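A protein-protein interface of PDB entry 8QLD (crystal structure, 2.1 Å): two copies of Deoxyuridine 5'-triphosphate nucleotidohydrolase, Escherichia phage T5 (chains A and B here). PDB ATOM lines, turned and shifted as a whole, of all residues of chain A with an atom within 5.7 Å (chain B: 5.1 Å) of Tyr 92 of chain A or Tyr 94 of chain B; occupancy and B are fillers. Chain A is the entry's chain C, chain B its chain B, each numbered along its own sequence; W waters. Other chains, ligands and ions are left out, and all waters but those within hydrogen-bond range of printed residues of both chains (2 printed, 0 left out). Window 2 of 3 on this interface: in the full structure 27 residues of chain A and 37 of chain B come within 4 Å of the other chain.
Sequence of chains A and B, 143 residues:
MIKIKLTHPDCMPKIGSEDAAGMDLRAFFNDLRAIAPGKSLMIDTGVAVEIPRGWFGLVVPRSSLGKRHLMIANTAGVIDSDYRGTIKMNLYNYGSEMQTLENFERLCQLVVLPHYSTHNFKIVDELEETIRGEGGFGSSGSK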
ATOM      1  N   ILE A  35     -12.163  -1.025 -27.302  1.00  0.00           N
ATOM      2  CA  ILE A  35     -12.472   0.379 -27.408  1.00  0.00           C
ATOM      3  C   ILE A  35     -12.158   0.769 -28.834  1.00  0.00           C
ATOM      4  O   ILE A  35     -10.994   0.804 -29.212  1.00  0.00           O
ATOM      5  CB  ILE A  35     -11.721   1.232 -26.365  1.00  0.00           C
ATOM      6  CG1 ILE A  35     -11.796   0.625 -24.963  1.00  0.00           C
ATOM      7  CG2 ILE A  35     -12.286   2.633 -26.373  1.00  0.00           C
ATOM      8  CD1 ILE A  35     -10.897   1.278 -23.952  1.00  0.00           C
ATOM      9  N   PRO A  37     -11.967   3.339 -32.116  1.00  0.00           N
ATOM     10  CA  PRO A  37     -11.641   4.743 -32.339  1.00  0.00           C
ATOM     11  C   PRO A  37     -12.883   5.611 -32.189  1.00  0.00           C
ATOM     12  O   PRO A  37     -13.918   5.311 -32.757  1.00  0.00           O
ATOM     13  CB  PRO A  37     -11.141   4.822 -33.788  1.00  0.00           C
ATOM     14  CG  PRO A  37     -10.808   3.396 -34.183  1.00  0.00           C
ATOM     15  CD  PRO A  37     -11.564   2.487 -33.240  1.00  0.00           C
ATOM     16  N   GLY A  38     -12.766   6.666 -31.380  1.00  0.00           N
ATOM     17  CA  GLY A  38     -13.834   7.619 -31.167  1.00  0.00           C
ATOM     18  C   GLY A  38     -14.867   7.120 -30.163  1.00  0.00           C
ATOM     19  O   GLY A  38     -15.882   7.781 -30.001  1.00  0.00           O
ATOM     20  N   LYS A  39     -14.612   5.995 -29.469  1.00  0.00           N
ATOM     21  CA  LYS A  39     -15.544   5.514 -28.445  1.00  0.00           C
ATOM     22  C   LYS A  39     -14.843   5.443 -27.086  1.00  0.00           C
ATOM     23  O   LYS A  39     -13.619   5.440 -27.018  1.00  0.00           O
ATOM     24  CB  LYS A  39     -16.140   4.142 -28.802  1.00  0.00           C
ATOM     25  CG  LYS A  39     -16.727   3.954 -30.199  1.00  0.00           C
ATOM     26  CD  LYS A  39     -18.037   4.667 -30.472  1.00  0.00           C
ATOM     27  CE  LYS A  39     -17.931   5.738 -31.548  1.00  0.00           C
ATOM     28  NZ  LYS A  39     -18.988   6.777 -31.446  1.00  0.00           N
ATOM     29  N   SER A  40     -15.635   5.403 -26.004  1.00  0.00           N
ATOM     30  CA  SER A  40     -15.115   5.236 -24.658  1.00  0.00           C
ATOM     31  C   SER A  40     -15.848   4.099 -23.967  1.00  0.00           C
ATOM     32  O   SER A  40     -17.033   3.906 -24.206  1.00  0.00           O
ATOM     33  CB  SER A  40     -15.207   6.499 -23.839  1.00  0.00           C
ATOM     34  OG  SER A  40     -16.431   7.187 -24.079  1.00  0.00           O
ATOM     35  N   LEU A  41     -15.122   3.349 -23.128  1.00  0.00           N
ATOM     36  CA  LEU A  41     -15.703   2.311 -22.290  1.00  0.00           C
ATOM     37  C   LEU A  41     -15.246   2.556 -20.862  1.00  0.00           C
ATOM     38  O   LEU A  41     -14.062   2.791 -20.619  1.00  0.00           O
ATOM     39  CB  LEU A  41     -15.259   0.917 -22.747  1.00  0.00           C
ATOM     40  CG  LEU A  41     -16.106   0.209 -23.805  1.00  0.00           C
ATOM     41  CD1 LEU A  41     -15.522  -1.160 -24.101  1.00  0.00           C
ATOM     42  CD2 LEU A  41     -17.575   0.057 -23.396  1.00  0.00           C
ATOM     43  N   HIS A  69      -2.875   5.348 -27.651  1.00  0.00           N
ATOM     44  CA  HIS A  69      -3.832   6.422 -27.886  1.00  0.00           C
ATOM     45  C   HIS A  69      -5.116   6.206 -27.092  1.00  0.00           C
ATOM     46  O   HIS A  69      -6.227   6.351 -27.604  1.00  0.00           O
ATOM     47  CB  HIS A  69      -4.079   6.619 -29.380  1.00  0.00           C
ATOM     48  CG  HIS A  69      -2.859   6.958 -30.158  1.00  0.00           C
ATOM     49  ND1 HIS A  69      -1.868   7.827 -29.738  1.00  0.00           N
ATOM     50  CD2 HIS A  69      -2.473   6.508 -31.365  1.00  0.00           C
ATOM     51  CE1 HIS A  69      -0.939   7.903 -30.693  1.00  0.00           C
ATOM     52  NE2 HIS A  69      -1.282   7.075 -31.676  1.00  0.00           N
ATOM     53  N   LEU A  70      -4.944   5.867 -25.815  1.00  0.00           N
ATOM     54  CA  LEU A  70      -6.030   5.856 -24.848  1.00  0.00           C
ATOM     55  C   LEU A  70      -5.824   7.015 -23.887  1.00  0.00           C
ATOM     56  O   LEU A  70      -4.698   7.233 -23.440  1.00  0.00           O
ATOM     57  CB  LEU A  70      -6.015   4.552 -24.060  1.00  0.00           C
ATOM     58  CG  LEU A  70      -6.456   3.310 -24.834  1.00  0.00           C
ATOM     59  CD1 LEU A  70      -6.211   2.072 -24.008  1.00  0.00           C
ATOM     60  CD2 LEU A  70      -7.895   3.417 -25.235  1.00  0.00           C
ATOM     61  N   MET A  71      -6.923   7.716 -23.594  1.00  0.00           N
ATOM     62  CA  MET A  71      -6.967   8.677 -22.520  1.00  0.00           C
ATOM     63  C   MET A  71      -8.202   8.398 -21.674  1.00  0.00           C
ATOM     64  O   MET A  71      -9.126   7.698 -22.065  1.00  0.00           O
ATOM     65  CB  MET A  71      -7.013  10.122 -23.025  1.00  0.00           C
ATOM     66  CG  MET A  71      -8.159  10.386 -23.953  1.00  0.00           C
ATOM     67  SD  MET A  71      -8.260  12.070 -24.587  1.00  0.00           S
ATOM     68  CE  MET A  71      -8.824  12.914 -23.112  1.00  0.00           C
ATOM     69  N   ILE A  72      -8.168   8.907 -20.449  1.00  0.00           N
ATOM     70  CA  ILE A  72      -9.350   8.951 -19.610  1.00  0.00           C
ATOM     71  C   ILE A  72     -10.266   9.981 -20.247  1.00  0.00           C
ATOM     72  O   ILE A  72      -9.788  11.043 -20.651  1.00  0.00           O
ATOM     73  CB  ILE A  72      -8.938   9.288 -18.169  1.00  0.00           C
ATOM     74  CG1 ILE A  72      -8.249   8.066 -17.559  1.00  0.00           C
ATOM     75  CG2 ILE A  72     -10.113   9.750 -17.309  1.00  0.00           C
ATOM     76  CD1 ILE A  72      -7.342   8.402 -16.414  1.00  0.00           C
ATOM     77  N   ALA A  73     -11.560   9.620 -20.390  1.00  0.00           N
ATOM     78  CA  ALA A  73     -12.501  10.476 -21.102  1.00  0.00           C
ATOM     79  C   ALA A  73     -12.532  11.864 -20.469  1.00  0.00           C
ATOM     80  O   ALA A  73     -12.584  12.854 -21.182  1.00  0.00           O
ATOM     81  CB  ALA A  73     -13.876   9.858 -21.108  1.00  0.00           C
ATOM     82  N   ASN A  74     -12.541  11.907 -19.127  1.00  0.00           N
ATOM     83  CA  ASN A  74     -12.634  13.140 -18.347  1.00  0.00           C
ATOM     84  C   ASN A  74     -11.247  13.693 -18.009  1.00  0.00           C
ATOM     85  O   ASN A  74     -11.111  14.490 -17.084  1.00  0.00           O
ATOM     86  CB  ASN A  74     -13.443  12.933 -17.068  1.00  0.00           C
ATOM     87  CG  ASN A  74     -13.127  11.658 -16.304  1.00  0.00           C
ATOM     88  OD1 ASN A  74     -13.213  10.525 -16.819  1.00  0.00           O
ATOM     89  ND2 ASN A  74     -12.806  11.846 -15.033  1.00  0.00           N
ATOM     90  N   ASN A  90     -12.802   5.521 -17.283  1.00  0.00           N
ATOM     91  CA  ASN A  90     -13.540   5.743 -18.512  1.00  0.00           C
ATOM     92  C   ASN A  90     -12.533   6.014 -19.635  1.00  0.00           C
ATOM     93  O   ASN A  90     -12.068   7.147 -19.825  1.00  0.00           O
ATOM     94  CB  ASN A  90     -14.548   6.880 -18.356  1.00  0.00           C
ATOM     95  CG  ASN A  90     -15.575   6.952 -19.467  1.00  0.00           C
ATOM     96  OD1 ASN A  90     -15.793   5.994 -20.211  1.00  0.00           O
ATOM     97  ND2 ASN A  90     -16.236   8.085 -19.578  1.00  0.00           N
ATOM     98  N   LEU A  91     -12.185   4.956 -20.379  1.00  0.00           N
ATOM     99  CA  LEU A  91     -11.079   5.059 -21.318  1.00  0.00           C
ATOM    100  C   LEU A  91     -11.603   5.292 -22.728  1.00  0.00           C
ATOM    101  O   LEU A  91     -12.412   4.520 -23.233  1.00  0.00           O
ATOM    102  CB  LEU A  91     -10.218   3.795 -21.210  1.00  0.00           C
ATOM    103  CG  LEU A  91      -9.368   3.677 -19.941  1.00  0.00           C
ATOM    104  CD1 LEU A  91      -8.597   2.372 -19.929  1.00  0.00           C
ATOM    105  CD2 LEU A  91      -8.423   4.853 -19.779  1.00  0.00           C
ATOM    106  N   TYR A  92     -11.079   6.334 -23.375  1.00  0.00           N
ATOM    107  CA  TYR A  92     -11.462   6.724 -24.712  1.00  0.00           C
ATOM    108  C   TYR A  92     -10.293   6.513 -25.686  1.00  0.00           C
ATOM    109  O   TYR A  92      -9.133   6.833 -25.393  1.00  0.00           O
ATOM    110  CB  TYR A  92     -11.810   8.217 -24.667  1.00  0.00           C
ATOM    111  CG  TYR A  92     -12.098   8.861 -26.013  1.00  0.00           C
ATOM    112  CD1 TYR A  92     -13.372   8.817 -26.560  1.00  0.00           C
ATOM    113  CD2 TYR A  92     -11.097   9.476 -26.758  1.00  0.00           C
ATOM    114  CE1 TYR A  92     -13.651   9.392 -27.792  1.00  0.00           C
ATOM    115  CE2 TYR A  92     -11.355  10.032 -28.010  1.00  0.00           C
ATOM    116  CZ  TYR A  92     -12.642  10.007 -28.515  1.00  0.00           C
ATOM    117  OH  TYR A  92     -12.959  10.532 -29.738  1.00  0.00           O
ATOM    118  N   ASN A  93     -10.642   6.033 -26.878  1.00  0.00           N
ATOM    119  CA  ASN A  93      -9.669   5.714 -27.914  1.00  0.00           C
ATOM    120  C   ASN A  93      -9.637   6.894 -28.874  1.00  0.00           C
ATOM    121  O   ASN A  93     -10.567   7.058 -29.669  1.00  0.00           O
ATOM    122  CB  ASN A  93     -10.005   4.403 -28.625  1.00  0.00           C
ATOM    123  CG  ASN A  93      -9.003   4.010 -29.693  1.00  0.00           C
ATOM    124  OD1 ASN A  93      -8.095   4.772 -30.040  1.00  0.00           O
ATOM    125  ND2 ASN A  93      -9.150   2.797 -30.193  1.00  0.00           N
ATOM    126  N   TYR A  94      -8.593   7.731 -28.747  1.00  0.00           N
ATOM    127  CA  TYR A  94      -8.471   8.917 -29.577  1.00  0.00           C
ATOM    128  C   TYR A  94      -7.668   8.581 -30.823  1.00  0.00           C
ATOM    129  O   TYR A  94      -7.524   9.459 -31.659  1.00  0.00           O
ATOM    130  CB  TYR A  94      -7.873  10.134 -28.871  1.00  0.00           C
ATOM    131  CG  TYR A  94      -6.429  10.020 -28.408  1.00  0.00           C
ATOM    132  CD1 TYR A  94      -5.377  10.281 -29.269  1.00  0.00           C
ATOM    133  CD2 TYR A  94      -6.124   9.679 -27.094  1.00  0.00           C
ATOM    134  CE1 TYR A  94      -4.061  10.264 -28.819  1.00  0.00           C
ATOM    135  CE2 TYR A  94      -4.815   9.618 -26.648  1.00  0.00           C
ATOM    136  CZ  TYR A  94      -3.778   9.926 -27.504  1.00  0.00           C
ATOM    137  OH  TYR A  94      -2.483   9.817 -27.063  1.00  0.00           O
ATOM    138  N   GLY B  66     -16.712  13.680 -19.327  1.00  0.00           N
ATOM    139  CA  GLY B  66     -16.022  12.579 -19.968  1.00  0.00           C
ATOM    140  C   GLY B  66     -16.904  11.936 -21.027  1.00  0.00           C
ATOM    141  O   GLY B  66     -16.447  11.709 -22.159  1.00  0.00           O
ATOM    142  N   HIS B  69     -17.220  13.929 -24.088  1.00  0.00           N
ATOM    143  CA  HIS B  69     -16.031  13.960 -24.931  1.00  0.00           C
ATOM    144  C   HIS B  69     -15.516  15.383 -25.108  1.00  0.00           C
ATOM    145  O   HIS B  69     -15.235  15.810 -26.231  1.00  0.00           O
ATOM    146  CB  HIS B  69     -16.287  13.249 -26.264  1.00  0.00           C
ATOM    147  CG  HIS B  69     -16.425  11.782 -26.108  1.00  0.00           C
ATOM    148  ND1 HIS B  69     -17.122  11.027 -27.019  1.00  0.00           N
ATOM    149  CD2 HIS B  69     -16.031  10.938 -25.135  1.00  0.00           C
ATOM    150  CE1 HIS B  69     -17.095   9.750 -26.637  1.00  0.00           C
ATOM    151  NE2 HIS B  69     -16.452   9.674 -25.488  1.00  0.00           N
ATOM    152  N   LEU B  70     -15.387  16.079 -23.968  1.00  0.00           N
ATOM    153  CA  LEU B  70     -14.853  17.433 -23.893  1.00  0.00           C
ATOM    154  C   LEU B  70     -13.606  17.416 -23.012  1.00  0.00           C
ATOM    155  O   LEU B  70     -13.579  16.780 -21.941  1.00  0.00           O
ATOM    156  CB  LEU B  70     -15.894  18.391 -23.288  1.00  0.00           C
ATOM    157  CG  LEU B  70     -17.048  18.841 -24.188  1.00  0.00           C
ATOM    158  CD1 LEU B  70     -18.118  19.596 -23.393  1.00  0.00           C
ATOM    159  CD2 LEU B  70     -16.519  19.706 -25.324  1.00  0.00           C
ATOM    160  N   MET B  71     -12.588  18.149 -23.476  1.00  0.00           N
ATOM    161  CA  MET B  71     -11.389  18.327 -22.692  1.00  0.00           C
ATOM    162  C   MET B  71     -11.006  19.797 -22.681  1.00  0.00           C
ATOM    163  O   MET B  71     -11.436  20.610 -23.508  1.00  0.00           O
ATOM    164  CB  MET B  71     -10.210  17.518 -23.245  1.00  0.00           C
ATOM    165  CG  MET B  71     -10.075  17.632 -24.731  1.00  0.00           C
ATOM    166  SD  MET B  71      -8.495  17.053 -25.367  1.00  0.00           S
ATOM    167  CE  MET B  71      -8.302  15.485 -24.545  1.00  0.00           C
ATOM    168  N   TYR B  92     -12.440  21.912 -25.527  1.00  0.00           N
ATOM    169  CA  TYR B  92     -12.358  21.361 -26.864  1.00  0.00           C
ATOM    170  C   TYR B  92     -13.174  20.070 -26.938  1.00  0.00           C
ATOM    171  O   TYR B  92     -13.101  19.221 -26.038  1.00  0.00           O
ATOM    172  CB  TYR B  92     -10.885  21.101 -27.177  1.00  0.00           C
ATOM    173  CG  TYR B  92     -10.640  20.435 -28.520  1.00  0.00           C
ATOM    174  CD1 TYR B  92     -10.512  21.189 -29.678  1.00  0.00           C
ATOM    175  CD2 TYR B  92     -10.600  19.052 -28.635  1.00  0.00           C
ATOM    176  CE1 TYR B  92     -10.307  20.586 -30.907  1.00  0.00           C
ATOM    177  CE2 TYR B  92     -10.391  18.440 -29.857  1.00  0.00           C
ATOM    178  CZ  TYR B  92     -10.232  19.210 -30.993  1.00  0.00           C
ATOM    179  OH  TYR B  92     -10.034  18.629 -32.202  1.00  0.00           O
ATOM    180  N   ASN B  93     -13.951  19.960 -28.024  1.00  0.00           N
ATOM    181  CA  ASN B  93     -14.770  18.798 -28.329  1.00  0.00           C
ATOM    182  C   ASN B  93     -13.944  17.837 -29.180  1.00  0.00           C
ATOM    183  O   ASN B  93     -13.703  18.085 -30.368  1.00  0.00           O
ATOM    184  CB  ASN B  93     -16.077  19.218 -28.998  1.00  0.00           C
ATOM    185  CG  ASN B  93     -17.048  18.071 -29.207  1.00  0.00           C
ATOM    186  OD1 ASN B  93     -16.676  16.892 -29.159  1.00  0.00           O
ATOM    187  ND2 ASN B  93     -18.297  18.402 -29.479  1.00  0.00           N
ATOM    188  N   TYR B  94     -13.503  16.738 -28.552  1.00  0.00           N
ATOM    189  CA  TYR B  94     -12.727  15.739 -29.268  1.00  0.00           C
ATOM    190  C   TYR B  94     -13.613  14.631 -29.826  1.00  0.00           C
ATOM    191  O   TYR B  94     -13.091  13.717 -30.453  1.00  0.00           O
ATOM    192  CB  TYR B  94     -11.616  15.175 -28.387  1.00  0.00           C
ATOM    193  CG  TYR B  94     -12.044  14.410 -27.151  1.00  0.00           C
ATOM    194  CD1 TYR B  94     -12.421  13.084 -27.227  1.00  0.00           C
ATOM    195  CD2 TYR B  94     -12.088  15.026 -25.908  1.00  0.00           C
ATOM    196  CE1 TYR B  94     -12.781  12.369 -26.104  1.00  0.00           C
ATOM    197  CE2 TYR B  94     -12.474  14.337 -24.771  1.00  0.00           C
ATOM    198  CZ  TYR B  94     -12.815  12.997 -24.873  1.00  0.00           C
ATOM    199  OH  TYR B  94     -13.230  12.236 -23.823  1.00  0.00           O
ATOM    200  N   GLY B  95     -14.924  14.691 -29.566  1.00  0.00           N
ATOM    201  CA  GLY B  95     -15.836  13.619 -29.955  1.00  0.00           C
ATOM    202  C   GLY B  95     -16.425  13.847 -31.342  1.00  0.00           C
ATOM    203  O   GLY B  95     -15.906  14.643 -32.123  1.00  0.00           O
ATOM    204  N   SER B  96     -17.535  13.160 -31.640  1.00  0.00           N
ATOM    205  CA  SER B  96     -18.110  13.191 -32.981  1.00  0.00           C
ATOM    206  C   SER B  96     -19.497  13.828 -33.025  1.00  0.00           C
ATOM    207  O   SER B  96     -20.051  13.932 -34.099  1.00  0.00           O
ATOM    208  CB  SER B  96     -18.158  11.806 -33.579  1.00  0.00           C
ATOM    209  OG  SER B  96     -19.081  11.006 -32.863  1.00  0.00           O
HETATM  210  O   HOH W   1     -11.839  15.286 -20.687  1.00  0.00           O
HETATM  211  O   HOH W   2     -13.786  11.744 -32.206  1.00  0.00           O
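Among the printed residues, merely in contact across the chains: Met 71 of chain A with Met 71 of chain B (3.0 Å), Ala 73 of chain A with Gly 66 of chain B (3.3 Å), Tyr 92 of chain A with His 69 of chain B (3.4 Å) and Asn 74 of chain A with Gly 66 of chain B (3.6 Å).
Of the 17 printed residues of chain A, 5 touch a printed residue of chain B.
Hydrophobic or aromatic side chains of chain B within 4 Å of the printed part of chain A: His 69, Met 71 and Tyr 94.
Among the printed residues, no Asp or Glu carboxylate lies within 4 Å of a Lys or Arg side-chain nitrogen of the other chain.
Of chain B, only His 69 and Tyr 94 come within 4 Å of Tyr 92 of chain A.
Tyr 94 of chain B touches just these residues of chain A: Ala 73 (2.8 Å) and Tyr 92 (3.3 Å).
Of the printed residues of chain A, Met 71 of chain B touches Met 71 (3.0 Å).
Of the printed residues of chain A, Gly 66 of chain B touches Ala 73 (3.3 Å) and Asn 74 (3.6 Å).
Of the printed residues of chain A, His 69 of chain B touches Ser 40 and Tyr 92.
Printed residues of chain B within 4 Å of Met 71 of chain A: Met 71 (3.0 Å).
Pro 37 of chain A touches none of the printed residues of chain B.
Asn 93 of chain A touches none of the printed residues of chain B.
The nearest residue of chain A that does not touch Tyr 94 of chain B is Met 71 of chain A (4.3 Å).
The nearest printed residue of chain B that does not touch Ala 73 of chain A is Leu 70 of chain B (4.1 Å).
Water W1 bridges the backbone carbonyl oxygen of Ala 73 of chain A (2.6 Å) and the backbone carbonyl oxygen of Leu 70 of chain B (2.6 Å).
Water W2 lies within hydrogen-bond range of O of Tyr 94 of chain B and OH of Tyr 92 of chain A.
The backbone carbonyl oxygen (O) of Met 71 of chain A sits at hydrogen-bond distance from the backbone NH (N) of Tyr 92 of chain A (2.7 Å).
N of Tyr 92 of chain B sits at hydrogen-bond distance from O of Met 71 of chain B.
The backbone NH of Tyr 94 of chain B sits at hydrogen-bond distance from the backbone carbonyl oxygen of His 69 of chain B (3.0 Å).
The backbone NH (N) of Ala 73 of chain A lies within hydrogen-bond range of the backbone carbonyl oxygen (O) of Asn 90 of chain A.
O of His 69 of chain B sits close to OD1 of Asn 93 of chain B.
Met 71 of chain A touches its own counterpart, Met 71 of chain B.
Tyr 92 of chain A touches His 69 of chain B, but with the chains exchanged His 69 of chain A does not touch Tyr 92 of chain B (13.0 Å).
Tyr 92 of chain A touches Tyr 94 of chain B, but with the chains exchanged Tyr 94 of chain A does not touch Tyr 92 of chain B (8.7 Å).
Positions printed for both chains: 69, 70, 71, 92, 93 and 94.
The side-chain hydroxyl (OH) of Tyr 92 of chain A lies within hydrogen-bond range of the backbone carbonyl oxygen (O) of Tyr 94 of chain B, 3.3 Å away.
OH of Tyr 94 of chain B is in hydrogen-bond range of O of Ala 73 of chain A (2.8 Å).
A ring nitrogen (NE2) of His 69 of chain B sits at hydrogen-bond distance from the side-chain hydroxyl of Ser 40 of chain A.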
